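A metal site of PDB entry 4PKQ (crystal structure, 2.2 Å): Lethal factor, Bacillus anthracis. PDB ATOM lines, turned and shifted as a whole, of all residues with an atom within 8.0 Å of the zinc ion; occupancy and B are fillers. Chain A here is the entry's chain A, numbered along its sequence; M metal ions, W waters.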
ATOM      1  N   ASP A  67       9.143  18.842 -16.416  1.00  0.00           N
ATOM      2  CA  ASP A  67       9.539  18.108 -17.622  1.00  0.00           C
ATOM      3  C   ASP A  67       8.331  17.689 -18.473  1.00  0.00           C
ATOM      4  O   ASP A  67       8.450  16.839 -19.362  1.00  0.00           O
ATOM      5  CB  ASP A  67      10.382  16.870 -17.244  1.00  0.00           C
ATOM      6  CG  ASP A  67       9.608  15.849 -16.398  1.00  0.00           C
ATOM      7  OD1 ASP A  67       8.499  16.146 -15.908  1.00  0.00           O
ATOM      8  OD2 ASP A  67      10.139  14.725 -16.218  1.00  0.00           O
ATOM      9  N   SER A 394       7.249  17.047 -24.357  1.00  0.00           N
ATOM     10  CA  SER A 394       8.704  17.107 -24.209  1.00  0.00           C
ATOM     11  C   SER A 394       9.384  16.685 -25.507  1.00  0.00           C
ATOM     12  O   SER A 394       8.727  16.393 -26.492  1.00  0.00           O
ATOM     13  CB  SER A 394       9.214  16.220 -23.046  1.00  0.00           C
ATOM     14  OG  SER A 394       8.936  14.861 -23.249  1.00  0.00           O
ATOM     15  N   GLY A 396      11.055  13.981 -25.970  1.00  0.00           N
ATOM     16  CA  GLY A 396      10.786  12.577 -26.214  1.00  0.00           C
ATOM     17  C   GLY A 396       9.952  11.903 -25.140  1.00  0.00           C
ATOM     18  O   GLY A 396       9.746  12.452 -24.053  1.00  0.00           O
ATOM     19  N   LEU A 397       9.479  10.698 -25.421  1.00  0.00           N
ATOM     20  CA  LEU A 397       8.696   9.944 -24.454  1.00  0.00           C
ATOM     21  C   LEU A 397       8.735   8.464 -24.775  1.00  0.00           C
ATOM     22  O   LEU A 397       8.786   8.087 -25.933  1.00  0.00           O
ATOM     23  CB  LEU A 397       7.258  10.429 -24.439  1.00  0.00           C
ATOM     24  CG  LEU A 397       6.244   9.973 -23.389  1.00  0.00           C
ATOM     25  CD1 LEU A 397       6.643  10.447 -21.996  1.00  0.00           C
ATOM     26  CD2 LEU A 397       4.836  10.497 -23.755  1.00  0.00           C
ATOM     27  N   TYR A 398       8.695   7.629 -23.748  1.00  0.00           N
ATOM     28  CA  TYR A 398       8.439   6.226 -23.989  1.00  0.00           C
ATOM     29  C   TYR A 398       7.141   5.864 -23.295  1.00  0.00           C
ATOM     30  O   TYR A 398       6.941   6.197 -22.138  1.00  0.00           O
ATOM     31  CB  TYR A 398       9.585   5.330 -23.480  1.00  0.00           C
ATOM     32  CG  TYR A 398       9.240   3.841 -23.568  1.00  0.00           C
ATOM     33  CD1 TYR A 398       9.177   3.195 -24.797  1.00  0.00           C
ATOM     34  CD2 TYR A 398       8.952   3.108 -22.422  1.00  0.00           C
ATOM     35  CE1 TYR A 398       8.845   1.853 -24.882  1.00  0.00           C
ATOM     36  CE2 TYR A 398       8.616   1.768 -22.497  1.00  0.00           C
ATOM     37  CZ  TYR A 398       8.573   1.145 -23.725  1.00  0.00           C
ATOM     38  OH  TYR A 398       8.253  -0.182 -23.809  1.00  0.00           O
ATOM     39  N   GLY A 422      18.572  12.093 -27.473  1.00  0.00           N
ATOM     40  CA  GLY A 422      17.211  12.026 -26.966  1.00  0.00           C
ATOM     41  C   GLY A 422      16.530  10.697 -27.270  1.00  0.00           C
ATOM     42  O   GLY A 422      15.783  10.166 -26.446  1.00  0.00           O
ATOM     43  N   HIS A 425      18.084   8.038 -24.930  1.00  0.00           N
ATOM     44  CA  HIS A 425      17.488   8.164 -23.609  1.00  0.00           C
ATOM     45  C   HIS A 425      16.165   7.396 -23.547  1.00  0.00           C
ATOM     46  O   HIS A 425      15.945   6.585 -22.630  1.00  0.00           O
ATOM     47  CB  HIS A 425      17.276   9.645 -23.243  1.00  0.00           C
ATOM     48  CG  HIS A 425      16.442   9.871 -22.011  1.00  0.00           C
ATOM     49  ND1 HIS A 425      16.986  10.266 -20.804  1.00  0.00           N
ATOM     50  CD2 HIS A 425      15.105   9.793 -21.814  1.00  0.00           C
ATOM     51  CE1 HIS A 425      16.023  10.401 -19.908  1.00  0.00           C
ATOM     52  NE2 HIS A 425      14.871  10.111 -20.494  1.00  0.00           N
ATOM     53  N   GLU A 426      15.304   7.631 -24.534  1.00  0.00           N
ATOM     54  CA  GLU A 426      13.988   6.990 -24.550  1.00  0.00           C
ATOM     55  C   GLU A 426      14.120   5.479 -24.710  1.00  0.00           C
ATOM     56  O   GLU A 426      13.332   4.701 -24.164  1.00  0.00           O
ATOM     57  CB  GLU A 426      13.100   7.566 -25.660  1.00  0.00           C
ATOM     58  CG  GLU A 426      12.893   9.092 -25.610  1.00  0.00           C
ATOM     59  CD  GLU A 426      12.370   9.614 -24.257  1.00  0.00           C
ATOM     60  OE1 GLU A 426      12.547  10.821 -23.997  1.00  0.00           O
ATOM     61  OE2 GLU A 426      11.796   8.845 -23.461  1.00  0.00           O
ATOM     62  N   PHE A 427      15.129   5.051 -25.466  1.00  0.00           N
ATOM     63  CA  PHE A 427      15.409   3.637 -25.615  1.00  0.00           C
ATOM     64  C   PHE A 427      15.821   3.051 -24.257  1.00  0.00           C
ATOM     65  O   PHE A 427      15.522   1.892 -23.957  1.00  0.00           O
ATOM     66  CB  PHE A 427      16.490   3.406 -26.669  1.00  0.00           C
ATOM     67  CG  PHE A 427      16.664   1.971 -27.045  1.00  0.00           C
ATOM     68  CD1 PHE A 427      15.737   1.338 -27.876  1.00  0.00           C
ATOM     69  CD2 PHE A 427      17.727   1.225 -26.561  1.00  0.00           C
ATOM     70  CE1 PHE A 427      15.893  -0.004 -28.224  1.00  0.00           C
ATOM     71  CE2 PHE A 427      17.882  -0.117 -26.909  1.00  0.00           C
ATOM     72  CZ  PHE A 427      16.962  -0.729 -27.742  1.00  0.00           C
ATOM     73  N   GLY A 428      16.504   3.851 -23.436  1.00  0.00           N
ATOM     74  CA  GLY A 428      16.782   3.444 -22.060  1.00  0.00           C
ATOM     75  C   GLY A 428      15.516   3.028 -21.324  1.00  0.00           C
ATOM     76  O   GLY A 428      15.492   1.991 -20.642  1.00  0.00           O
ATOM     77  N   HIS A 429      14.440   3.788 -21.486  1.00  0.00           N
ATOM     78  CA  HIS A 429      13.164   3.436 -20.852  1.00  0.00           C
ATOM     79  C   HIS A 429      12.606   2.088 -21.361  1.00  0.00           C
ATOM     80  O   HIS A 429      12.032   1.319 -20.596  1.00  0.00           O
ATOM     81  CB  HIS A 429      12.122   4.537 -21.088  1.00  0.00           C
ATOM     82  CG  HIS A 429      12.386   5.786 -20.313  1.00  0.00           C
ATOM     83  ND1 HIS A 429      12.546   5.807 -18.944  1.00  0.00           N
ATOM     84  CD2 HIS A 429      12.483   7.079 -20.710  1.00  0.00           C
ATOM     85  CE1 HIS A 429      12.733   7.041 -18.539  1.00  0.00           C
ATOM     86  NE2 HIS A 429      12.709   7.839 -19.587  1.00  0.00           N
ATOM     87  N   TYR A 467      18.960  16.199 -14.478  1.00  0.00           N
ATOM     88  CA  TYR A 467      17.675  15.594 -14.822  1.00  0.00           C
ATOM     89  C   TYR A 467      17.578  14.153 -14.308  1.00  0.00           C
ATOM     90  O   TYR A 467      16.478  13.648 -14.027  1.00  0.00           O
ATOM     91  CB  TYR A 467      17.439  15.629 -16.341  1.00  0.00           C
ATOM     92  CG  TYR A 467      16.060  15.118 -16.701  1.00  0.00           C
ATOM     93  CD1 TYR A 467      14.922  15.851 -16.365  1.00  0.00           C
ATOM     94  CD2 TYR A 467      15.887  13.907 -17.362  1.00  0.00           C
ATOM     95  CE1 TYR A 467      13.648  15.393 -16.674  1.00  0.00           C
ATOM     96  CE2 TYR A 467      14.603  13.431 -17.681  1.00  0.00           C
ATOM     97  CZ  TYR A 467      13.489  14.183 -17.332  1.00  0.00           C
ATOM     98  OH  TYR A 467      12.221  13.746 -17.643  1.00  0.00           O
ATOM     99  N   ASN A 471      13.917  10.859 -10.744  1.00  0.00           N
ATOM    100  CA  ASN A 471      13.442   9.605 -10.156  1.00  0.00           C
ATOM    101  C   ASN A 471      14.211   8.431 -10.726  1.00  0.00           C
ATOM    102  O   ASN A 471      15.020   8.611 -11.637  1.00  0.00           O
ATOM    103  CB  ASN A 471      11.926   9.391 -10.395  1.00  0.00           C
ATOM    104  CG  ASN A 471      11.556   9.393 -11.871  1.00  0.00           C
ATOM    105  OD1 ASN A 471      12.309   8.923 -12.723  1.00  0.00           O
ATOM    106  ND2 ASN A 471      10.379   9.942 -12.176  1.00  0.00           N
ATOM    107  N   ALA A 473      13.438   6.000 -12.795  1.00  0.00           N
ATOM    108  CA  ALA A 473      13.321   5.681 -14.205  1.00  0.00           C
ATOM    109  C   ALA A 473      14.183   6.626 -15.020  1.00  0.00           C
ATOM    110  O   ALA A 473      14.895   6.205 -15.905  1.00  0.00           O
ATOM    111  CB  ALA A 473      11.859   5.754 -14.659  1.00  0.00           C
ATOM    112  N   GLU A 474      14.134   7.917 -14.694  1.00  0.00           N
ATOM    113  CA  GLU A 474      14.893   8.909 -15.443  1.00  0.00           C
ATOM    114  C   GLU A 474      16.393   8.743 -15.212  1.00  0.00           C
ATOM    115  O   GLU A 474      17.188   8.961 -16.114  1.00  0.00           O
ATOM    116  CB  GLU A 474      14.451  10.335 -15.077  1.00  0.00           C
ATOM    117  CG  GLU A 474      12.962  10.620 -15.235  1.00  0.00           C
ATOM    118  CD  GLU A 474      12.451  10.399 -16.640  1.00  0.00           C
ATOM    119  OE1 GLU A 474      13.245  10.501 -17.603  1.00  0.00           O
ATOM    120  OE2 GLU A 474      11.251  10.110 -16.794  1.00  0.00           O
ATOM    121  N   PHE A 475      16.759   8.358 -13.984  1.00  0.00           N
ATOM    122  CA  PHE A 475      18.165   8.138 -13.620  1.00  0.00           C
ATOM    123  C   PHE A 475      18.749   7.011 -14.455  1.00  0.00           C
ATOM    124  O   PHE A 475      19.818   7.157 -15.030  1.00  0.00           O
ATOM    125  CB  PHE A 475      18.311   7.839 -12.124  1.00  0.00           C
ATOM    126  CG  PHE A 475      19.756   7.688 -11.657  1.00  0.00           C
ATOM    127  CD1 PHE A 475      20.640   8.739 -11.788  1.00  0.00           C
ATOM    128  CD2 PHE A 475      20.212   6.498 -11.113  1.00  0.00           C
ATOM    129  CE1 PHE A 475      21.963   8.601 -11.369  1.00  0.00           C
ATOM    130  CE2 PHE A 475      21.515   6.351 -10.698  1.00  0.00           C
ATOM    131  CZ  PHE A 475      22.406   7.409 -10.829  1.00  0.00           C
ATOM    132  N   ALA A 477      17.618   5.953 -17.270  1.00  0.00           N
ATOM    133  CA  ALA A 477      17.597   6.314 -18.681  1.00  0.00           C
ATOM    134  C   ALA A 477      18.757   7.228 -19.022  1.00  0.00           C
ATOM    135  O   ALA A 477      19.388   7.078 -20.073  1.00  0.00           O
ATOM    136  CB  ALA A 477      16.251   6.969 -19.057  1.00  0.00           C
ATOM    137  N   GLU A 478      19.039   8.170 -18.134  1.00  0.00           N
ATOM    138  CA  GLU A 478      20.177   9.085 -18.280  1.00  0.00           C
ATOM    139  C   GLU A 478      21.511   8.317 -18.202  1.00  0.00           C
ATOM    140  O   GLU A 478      22.410   8.523 -19.019  1.00  0.00           O
ATOM    141  CB  GLU A 478      20.119  10.165 -17.189  1.00  0.00           C
ATOM    142  CG  GLU A 478      19.140  11.293 -17.477  1.00  0.00           C
ATOM    143  CD  GLU A 478      19.560  12.152 -18.644  1.00  0.00           C
ATOM    144  OE1 GLU A 478      20.137  13.229 -18.402  1.00  0.00           O
ATOM    145  OE2 GLU A 478      19.315  11.764 -19.821  1.00  0.00           O
HETATM  146 ZN    ZN M   1      12.785  10.007 -19.678  1.00  0.00          ZN
HETATM  147  O   HOH W   1      12.267  12.388 -20.112  1.00  0.00           O
HETATM  148  O   HOH W   2      11.176  10.111 -21.402  1.00  0.00           O
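NE2 of His 429 binds the zinc ion (2.2 Å).
The zinc ion is bound by OE1 of Glu 474, 2.2 Å away.
The zinc ion is bound by NE2 of His 425 (2.2 Å).
The zinc ion is bound by water W2, at 2.4 Å.
The zinc ion is bound by water W1 (2.5 Å).
Of the 18 residues printed, 3 come within 4 Å of the zinc ion.
OH of Tyr 467 sits close to OE1 of Glu 474 (3.4 Å).
The side-chain amide oxygen (OD1) of Asn 471 is in hydrogen-bond range of the backbone NH (N) of Glu 474.
A ring nitrogen (ND1) of His 425 lies within hydrogen-bond range of the side-chain carboxylate of Glu 478, at 2.9 Å.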
